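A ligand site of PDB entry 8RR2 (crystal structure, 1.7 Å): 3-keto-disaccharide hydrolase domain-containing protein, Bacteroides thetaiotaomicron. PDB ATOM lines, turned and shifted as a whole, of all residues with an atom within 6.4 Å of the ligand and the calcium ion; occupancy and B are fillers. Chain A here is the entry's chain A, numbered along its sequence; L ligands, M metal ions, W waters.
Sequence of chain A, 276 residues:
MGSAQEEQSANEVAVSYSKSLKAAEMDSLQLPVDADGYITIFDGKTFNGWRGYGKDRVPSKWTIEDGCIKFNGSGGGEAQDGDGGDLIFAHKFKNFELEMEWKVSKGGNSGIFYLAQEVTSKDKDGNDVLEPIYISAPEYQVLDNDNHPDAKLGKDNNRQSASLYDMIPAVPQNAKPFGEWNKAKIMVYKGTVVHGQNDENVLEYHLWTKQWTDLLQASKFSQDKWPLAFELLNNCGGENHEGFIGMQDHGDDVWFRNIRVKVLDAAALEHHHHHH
The side-chain carboxylate of Glu 78 sits at hydrogen-bond distance from an oxygen (O6) of the ligand (2.5 Å).
O4 of the ligand is in hydrogen-bond range of NZ of Lys 220, at 2.9 Å.
OD2 of Asp 150 is in hydrogen-bond range of O2 of the ligand, 2.7 Å away.
O6 of the ligand is in hydrogen-bond range of NE2 of His 250 (2.7 Å).
The side-chain amide nitrogen of Gln 141 sits at hydrogen-bond distance from the side-chain carboxylate of Asp 150 (3.3 Å).
N of Gln 248 sits at hydrogen-bond distance from O of Gly 111, at 3.0 Å.
The backbone NH (N) of Lys 220 is in hydrogen-bond range of the side-chain carboxylate (OD2) of Asp 166.
The backbone NH of Asp 150 lies within hydrogen-bond range of a ring nitrogen (ND1) of His 148.
N of Ser 110 is in hydrogen-bond range of O of Val 142.
The side-chain amide nitrogen (ND2) of Asn 109 sits at hydrogen-bond distance from the side-chain carboxylate (OD2) of Asp 150.
O of Glu 139 lies within hydrogen-bond range of N of Tyr 165 (3.1 Å).
NE of Arg 159 sits close to OH of Tyr 165.
Tyr 134 touches the ligand (CG to C1, 3.5 Å).
OH of Tyr 165 touches C6 of the ligand, 3.2 Å away.
Phe 221 touches the ligand (CZ to O4, 3.9 Å).
Hydrophobic or aromatic side chains that line the ligand: Tyr 134, Tyr 165, Phe 221 and His 250.
Within 4 Å of the ligand: Glu 78, Asn 109, Tyr 134, Glu 139, Gln 141, Asp 150, Tyr 165, Lys 220, Phe 221, Gln 248 and His 250.
Of the 21 residues printed, 5 come within 4 Å of the calcium ion.
The calcium ion is bound by OE1 of Gln 141 (2.3 Å).
OE2 of Glu 139 is bound to the calcium ion, at 2.4 Å.
OE1 of Gln 248 is bound to the calcium ion (2.4 Å).
O of Ser 110 binds the calcium ion, 2.5 Å away.
O3 of the ligand is bound to the calcium ion.
The calcium ion is bound by OD1 of Asn 109.
The calcium ion is bound by O1 of the ligand (2.7 Å).
Water W2 lies within hydrogen-bond range of an oxygen (O2) of the ligand (2.6 Å) and the side-chain carboxylate (OD1) of Asp 150 (2.9 Å).
Water W1 bridges OE1 of Glu 139 (2.7 Å) and O4 of the ligand (2.7 Å).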
ATOM      1  N   GLY A  77     -13.308   0.744  16.552  1.00  0.00           N
ATOM      2  CA  GLY A  77     -13.701   0.863  17.948  1.00  0.00           C
ATOM      3  C   GLY A  77     -14.872  -0.031  18.318  1.00  0.00           C
ATOM      4  O   GLY A  77     -14.846  -1.256  18.135  1.00  0.00           O
ATOM      5  N   GLU A  78     -15.916   0.576  18.857  1.00  0.00           N
ATOM      6  CA  GLU A  78     -17.121  -0.179  19.251  1.00  0.00           C
ATOM      7  C   GLU A  78     -17.962  -0.626  18.068  1.00  0.00           C
ATOM      8  O   GLU A  78     -18.983  -1.294  18.281  1.00  0.00           O
ATOM      9  CB  GLU A  78     -18.000   0.670  20.169  1.00  0.00           C
ATOM     10  CG  GLU A  78     -17.472   0.860  21.591  1.00  0.00           C
ATOM     11  CD  GLU A  78     -18.513   1.538  22.486  1.00  0.00           C
ATOM     12  OE1 GLU A  78     -19.685   1.724  22.033  1.00  0.00           O
ATOM     13  OE2 GLU A  78     -18.145   1.919  23.611  1.00  0.00           O
ATOM     14  N   ASN A 109      -6.922  -1.635  21.860  1.00  0.00           N
ATOM     15  CA  ASN A 109      -7.885  -1.798  22.954  1.00  0.00           C
ATOM     16  C   ASN A 109      -8.585  -3.126  22.728  1.00  0.00           C
ATOM     17  O   ASN A 109      -9.004  -3.412  21.608  1.00  0.00           O
ATOM     18  CB  ASN A 109      -8.890  -0.611  22.970  1.00  0.00           C
ATOM     19  CG  ASN A 109     -10.026  -0.733  24.029  1.00  0.00           C
ATOM     20  OD1 ASN A 109     -10.497  -1.802  24.384  1.00  0.00           O
ATOM     21  ND2 ASN A 109     -10.453   0.421  24.542  1.00  0.00           N
ATOM     22  N   SER A 110      -8.728  -3.922  23.795  1.00  0.00           N
ATOM     23  CA  SER A 110      -9.604  -5.102  23.788  1.00  0.00           C
ATOM     24  C   SER A 110     -10.026  -5.312  25.241  1.00  0.00           C
ATOM     25  O   SER A 110     -10.105  -4.341  25.991  1.00  0.00           O
ATOM     26  CB  SER A 110      -8.875  -6.329  23.225  1.00  0.00           C
ATOM     27  OG  SER A 110      -9.720  -7.469  23.145  1.00  0.00           O
ATOM     28  N   GLY A 111     -10.314  -6.521  25.643  1.00  0.00           N
ATOM     29  CA  GLY A 111     -10.714  -6.750  27.029  1.00  0.00           C
ATOM     30  C   GLY A 111     -10.954  -8.230  27.226  1.00  0.00           C
ATOM     31  O   GLY A 111     -11.174  -8.975  26.273  1.00  0.00           O
ATOM     32  N   PHE A 113     -13.535 -10.607  29.231  1.00  0.00           N
ATOM     33  CA  PHE A 113     -14.796 -10.596  29.950  1.00  0.00           C
ATOM     34  C   PHE A 113     -14.944 -11.840  30.795  1.00  0.00           C
ATOM     35  O   PHE A 113     -14.373 -12.892  30.476  1.00  0.00           O
ATOM     36  CB  PHE A 113     -15.999 -10.534  28.991  1.00  0.00           C
ATOM     37  CG  PHE A 113     -16.027  -9.300  28.143  1.00  0.00           C
ATOM     38  CD1 PHE A 113     -16.341  -8.069  28.712  1.00  0.00           C
ATOM     39  CD2 PHE A 113     -15.752  -9.359  26.783  1.00  0.00           C
ATOM     40  CE1 PHE A 113     -16.349  -6.900  27.925  1.00  0.00           C
ATOM     41  CE2 PHE A 113     -15.780  -8.214  26.001  1.00  0.00           C
ATOM     42  CZ  PHE A 113     -16.081  -6.981  26.574  1.00  0.00           C
ATOM     43  N   TYR A 134     -20.790  -6.473  27.380  1.00  0.00           N
ATOM     44  CA  TYR A 134     -20.246  -5.781  28.543  1.00  0.00           C
ATOM     45  C   TYR A 134     -21.296  -5.163  29.443  1.00  0.00           C
ATOM     46  O   TYR A 134     -20.920  -4.633  30.497  1.00  0.00           O
ATOM     47  CB  TYR A 134     -19.233  -4.723  28.104  1.00  0.00           C
ATOM     48  CG  TYR A 134     -19.797  -3.675  27.189  1.00  0.00           C
ATOM     49  CD1 TYR A 134     -20.632  -2.667  27.662  1.00  0.00           C
ATOM     50  CD2 TYR A 134     -19.507  -3.689  25.813  1.00  0.00           C
ATOM     51  CE1 TYR A 134     -21.151  -1.684  26.803  1.00  0.00           C
ATOM     52  CE2 TYR A 134     -20.030  -2.699  24.959  1.00  0.00           C
ATOM     53  CZ  TYR A 134     -20.843  -1.714  25.473  1.00  0.00           C
ATOM     54  OH  TYR A 134     -21.386  -0.747  24.624  1.00  0.00           O
ATOM     55  N   GLU A 139     -15.369  -6.411  32.931  1.00  0.00           N
ATOM     56  CA  GLU A 139     -14.320  -6.427  31.926  1.00  0.00           C
ATOM     57  C   GLU A 139     -12.958  -6.154  32.572  1.00  0.00           C
ATOM     58  O   GLU A 139     -12.795  -5.165  33.279  1.00  0.00           O
ATOM     59  CB  GLU A 139     -14.624  -5.370  30.815  1.00  0.00           C
ATOM     60  CG  GLU A 139     -13.478  -5.327  29.832  1.00  0.00           C
ATOM     61  CD  GLU A 139     -13.602  -4.250  28.781  1.00  0.00           C
ATOM     62  OE1 GLU A 139     -14.634  -3.503  28.743  1.00  0.00           O
ATOM     63  OE2 GLU A 139     -12.643  -4.134  27.989  1.00  0.00           O
ATOM     64  N   TYR A 140     -12.002  -7.022  32.301  1.00  0.00           N
ATOM     65  CA  TYR A 140     -10.601  -6.746  32.566  1.00  0.00           C
ATOM     66  C   TYR A 140     -10.096  -6.023  31.321  1.00  0.00           C
ATOM     67  O   TYR A 140      -9.953  -6.631  30.261  1.00  0.00           O
ATOM     68  CB  TYR A 140      -9.887  -8.073  32.816  1.00  0.00           C
ATOM     69  CG  TYR A 140      -8.385  -8.110  32.990  1.00  0.00           C
ATOM     70  CD1 TYR A 140      -7.518  -7.797  31.946  1.00  0.00           C
ATOM     71  CD2 TYR A 140      -7.834  -8.554  34.189  1.00  0.00           C
ATOM     72  CE1 TYR A 140      -6.116  -7.874  32.124  1.00  0.00           C
ATOM     73  CE2 TYR A 140      -6.417  -8.662  34.382  1.00  0.00           C
ATOM     74  CZ  TYR A 140      -5.581  -8.313  33.325  1.00  0.00           C
ATOM     75  OH  TYR A 140      -4.215  -8.396  33.528  1.00  0.00           O
ATOM     76  N   GLN A 141      -9.881  -4.706  31.430  1.00  0.00           N
ATOM     77  CA  GLN A 141      -9.472  -3.917  30.276  1.00  0.00           C
ATOM     78  C   GLN A 141      -8.144  -4.414  29.732  1.00  0.00           C
ATOM     79  O   GLN A 141      -7.236  -4.758  30.488  1.00  0.00           O
ATOM     80  CB  GLN A 141      -9.324  -2.446  30.685  1.00  0.00           C
ATOM     81  CG  GLN A 141      -8.755  -1.541  29.611  1.00  0.00           C
ATOM     82  CD  GLN A 141      -9.762  -1.145  28.566  1.00  0.00           C
ATOM     83  OE1 GLN A 141     -10.379  -2.000  27.893  1.00  0.00           O
ATOM     84  NE2 GLN A 141      -9.945   0.159  28.395  1.00  0.00           N
ATOM     85  N   VAL A 142      -8.034  -4.433  28.412  1.00  0.00           N
ATOM     86  CA  VAL A 142      -6.790  -4.698  27.692  1.00  0.00           C
ATOM     87  C   VAL A 142      -6.484  -3.448  26.864  1.00  0.00           C
ATOM     88  O   VAL A 142      -7.336  -2.992  26.091  1.00  0.00           O
ATOM     89  CB  VAL A 142      -6.931  -5.954  26.814  1.00  0.00           C
ATOM     90  CG1 VAL A 142      -5.839  -6.043  25.702  1.00  0.00           C
ATOM     91  CG2 VAL A 142      -6.941  -7.203  27.698  1.00  0.00           C
ATOM     92  N   LEU A 143      -5.281  -2.901  27.020  1.00  0.00           N
ATOM     93  CA  LEU A 143      -5.059  -1.557  26.476  1.00  0.00           C
ATOM     94  C   LEU A 143      -3.575  -1.275  26.289  1.00  0.00           C
ATOM     95  O   LEU A 143      -2.737  -1.733  27.058  1.00  0.00           O
ATOM     96  CB  LEU A 143      -5.653  -0.496  27.409  1.00  0.00           C
ATOM     97  CG  LEU A 143      -5.815   0.877  26.743  1.00  0.00           C
ATOM     98  CD1 LEU A 143      -7.078   0.816  25.866  1.00  0.00           C
ATOM     99  CD2 LEU A 143      -5.978   1.972  27.739  1.00  0.00           C
ATOM    100  N   HIS A 148      -3.451   4.693  23.701  1.00  0.00           N
ATOM    101  CA  HIS A 148      -4.896   4.772  23.516  1.00  0.00           C
ATOM    102  C   HIS A 148      -5.497   5.828  24.453  1.00  0.00           C
ATOM    103  O   HIS A 148      -5.187   5.835  25.647  1.00  0.00           O
ATOM    104  CB  HIS A 148      -5.551   3.429  23.814  1.00  0.00           C
ATOM    105  CG  HIS A 148      -6.927   3.300  23.248  1.00  0.00           C
ATOM    106  ND1 HIS A 148      -8.009   4.006  23.741  1.00  0.00           N
ATOM    107  CD2 HIS A 148      -7.410   2.526  22.241  1.00  0.00           C
ATOM    108  CE1 HIS A 148      -9.097   3.684  23.051  1.00  0.00           C
ATOM    109  NE2 HIS A 148      -8.754   2.799  22.125  1.00  0.00           N
ATOM    110  N   ASP A 150      -8.277   6.063  26.003  1.00  0.00           N
ATOM    111  CA  ASP A 150      -8.899   5.533  27.229  1.00  0.00           C
ATOM    112  C   ASP A 150      -8.009   5.709  28.447  1.00  0.00           C
ATOM    113  O   ASP A 150      -8.507   5.870  29.580  1.00  0.00           O
ATOM    114  CB  ASP A 150      -9.217   4.031  27.124  1.00  0.00           C
ATOM    115  CG  ASP A 150     -10.544   3.779  26.502  1.00  0.00           C
ATOM    116  OD1 ASP A 150     -11.179   4.767  26.098  1.00  0.00           O
ATOM    117  OD2 ASP A 150     -10.948   2.593  26.439  1.00  0.00           O
ATOM    118  N   ARG A 159      -9.538   3.140  33.407  1.00  0.00           N
ATOM    119  CA  ARG A 159      -9.728   2.561  32.078  1.00  0.00           C
ATOM    120  C   ARG A 159      -8.421   2.049  31.490  1.00  0.00           C
ATOM    121  O   ARG A 159      -8.373   1.715  30.297  1.00  0.00           O
ATOM    122  CB  ARG A 159     -10.395   3.582  31.148  1.00  0.00           C
ATOM    123  CG  ARG A 159     -11.795   3.970  31.682  1.00  0.00           C
ATOM    124  CD  ARG A 159     -12.522   4.922  30.711  1.00  0.00           C
ATOM    125  NE  ARG A 159     -13.812   5.334  31.266  1.00  0.00           N
ATOM    126  CZ  ARG A 159     -14.666   6.140  30.634  1.00  0.00           C
ATOM    127  NH1 ARG A 159     -14.407   6.599  29.412  1.00  0.00           N
ATOM    128  NH2 ARG A 159     -15.804   6.478  31.240  1.00  0.00           N
ATOM    129  N   TYR A 165     -13.035  -2.223  34.146  1.00  0.00           N
ATOM    130  CA  TYR A 165     -13.299  -1.062  33.296  1.00  0.00           C
ATOM    131  C   TYR A 165     -14.316  -0.085  33.895  1.00  0.00           C
ATOM    132  O   TYR A 165     -15.446  -0.458  34.183  1.00  0.00           O
ATOM    133  CB  TYR A 165     -13.785  -1.501  31.897  1.00  0.00           C
ATOM    134  CG  TYR A 165     -13.947  -0.291  31.033  1.00  0.00           C
ATOM    135  CD1 TYR A 165     -12.870   0.260  30.344  1.00  0.00           C
ATOM    136  CD2 TYR A 165     -15.189   0.332  30.936  1.00  0.00           C
ATOM    137  CE1 TYR A 165     -13.038   1.421  29.595  1.00  0.00           C
ATOM    138  CE2 TYR A 165     -15.351   1.500  30.213  1.00  0.00           C
ATOM    139  CZ  TYR A 165     -14.273   2.018  29.535  1.00  0.00           C
ATOM    140  OH  TYR A 165     -14.416   3.162  28.785  1.00  0.00           O
ATOM    141  N   ASP A 166     -13.904   1.165  34.050  1.00  0.00           N
ATOM    142  CA  ASP A 166     -14.721   2.286  34.537  1.00  0.00           C
ATOM    143  C   ASP A 166     -15.089   2.163  35.988  1.00  0.00           C
ATOM    144  O   ASP A 166     -15.965   2.921  36.443  1.00  0.00           O
ATOM    145  CB  ASP A 166     -16.004   2.513  33.718  1.00  0.00           C
ATOM    146  CG  ASP A 166     -16.421   3.975  33.708  1.00  0.00           C
ATOM    147  OD1 ASP A 166     -15.526   4.848  33.595  1.00  0.00           O
ATOM    148  OD2 ASP A 166     -17.638   4.256  33.835  1.00  0.00           O
ATOM    149  N   LYS A 220     -20.478   4.181  34.246  1.00  0.00           N
ATOM    150  CA  LYS A 220     -21.301   4.275  33.050  1.00  0.00           C
ATOM    151  C   LYS A 220     -22.479   3.320  33.099  1.00  0.00           C
ATOM    152  O   LYS A 220     -23.410   3.448  32.272  1.00  0.00           O
ATOM    153  CB  LYS A 220     -20.474   3.953  31.788  1.00  0.00           C
ATOM    154  CG  LYS A 220     -19.871   2.543  31.801  1.00  0.00           C
ATOM    155  CD  LYS A 220     -18.948   2.278  30.615  1.00  0.00           C
ATOM    156  CE  LYS A 220     -19.710   2.232  29.305  1.00  0.00           C
ATOM    157  NZ  LYS A 220     -18.766   1.961  28.153  1.00  0.00           N
ATOM    158  N   PHE A 221     -22.448   2.337  33.997  1.00  0.00           N
ATOM    159  CA  PHE A 221     -23.511   1.344  34.101  1.00  0.00           C
ATOM    160  C   PHE A 221     -24.455   1.644  35.267  1.00  0.00           C
ATOM    161  O   PHE A 221     -25.112   0.732  35.772  1.00  0.00           O
ATOM    162  CB  PHE A 221     -22.928  -0.060  34.253  1.00  0.00           C
ATOM    163  CG  PHE A 221     -21.957  -0.445  33.162  1.00  0.00           C
ATOM    164  CD1 PHE A 221     -22.362  -0.524  31.845  1.00  0.00           C
ATOM    165  CD2 PHE A 221     -20.640  -0.754  33.484  1.00  0.00           C
ATOM    166  CE1 PHE A 221     -21.454  -0.883  30.827  1.00  0.00           C
ATOM    167  CE2 PHE A 221     -19.730  -1.135  32.496  1.00  0.00           C
ATOM    168  CZ  PHE A 221     -20.144  -1.202  31.177  1.00  0.00           C
ATOM    169  N   GLN A 248     -12.712  -9.261  23.695  1.00  0.00           N
ATOM    170  CA  GLN A 248     -13.441  -8.148  23.098  1.00  0.00           C
ATOM    171  C   GLN A 248     -12.991  -7.852  21.666  1.00  0.00           C
ATOM    172  O   GLN A 248     -11.779  -7.707  21.408  1.00  0.00           O
ATOM    173  CB  GLN A 248     -13.245  -6.883  23.939  1.00  0.00           C
ATOM    174  CG  GLN A 248     -14.129  -5.763  23.412  1.00  0.00           C
ATOM    175  CD  GLN A 248     -14.001  -4.537  24.273  1.00  0.00           C
ATOM    176  OE1 GLN A 248     -12.912  -4.176  24.671  1.00  0.00           O
ATOM    177  NE2 GLN A 248     -15.130  -3.941  24.629  1.00  0.00           N
ATOM    178  N   HIS A 250     -12.787  -4.771  19.857  1.00  0.00           N
ATOM    179  CA  HIS A 250     -12.836  -3.303  19.931  1.00  0.00           C
ATOM    180  C   HIS A 250     -12.108  -2.724  18.728  1.00  0.00           C
ATOM    181  O   HIS A 250     -11.529  -1.636  18.798  1.00  0.00           O
ATOM    182  CB  HIS A 250     -12.262  -2.781  21.246  1.00  0.00           C
ATOM    183  CG  HIS A 250     -12.793  -1.441  21.671  1.00  0.00           C
ATOM    184  ND1 HIS A 250     -12.185  -0.248  21.324  1.00  0.00           N
ATOM    185  CD2 HIS A 250     -13.891  -1.109  22.390  1.00  0.00           C
ATOM    186  CE1 HIS A 250     -12.893   0.761  21.822  1.00  0.00           C
ATOM    187  NE2 HIS A 250     -13.930   0.262  22.478  1.00  0.00           N
HETATM  188  C1  LIG L   1     -17.352  -1.117  27.087  1.00  0.00           C
HETATM  189  C2  LIG L   1     -15.568   1.732  25.556  1.00  0.00           C
HETATM  190  C3  LIG L   1     -13.794   0.112  26.279  1.00  0.00           C
HETATM  191  C4  LIG L   1     -14.870  -0.740  26.932  1.00  0.00           C
HETATM  192  C5  LIG L   1     -16.224  -0.448  26.320  1.00  0.00           C
HETATM  193  C6  LIG L   1     -14.125   1.578  26.030  1.00  0.00           C
HETATM  194  O1  LIG L   1     -14.512  -2.110  26.775  1.00  0.00           O
HETATM  195  O2  LIG L   1     -13.205   2.138  25.116  1.00  0.00           O
HETATM  196  O3  LIG L   1     -12.687  -0.336  26.078  1.00  0.00           O
HETATM  197  O4  LIG L   1     -17.479  -0.609  28.409  1.00  0.00           O
HETATM  198  O5  LIG L   1     -16.472   0.972  26.363  1.00  0.00           O
HETATM  199  O6  LIG L   1     -15.727   1.411  24.178  1.00  0.00           O
HETATM  200 CA    CA M   1     -11.905  -2.694  26.257  1.00  0.00          CA
HETATM  201  O   HOH W   1     -16.784  -2.606  30.122  1.00  0.00           O
HETATM  202  O   HOH W   2     -12.850   4.367  23.744  1.00  0.00           O
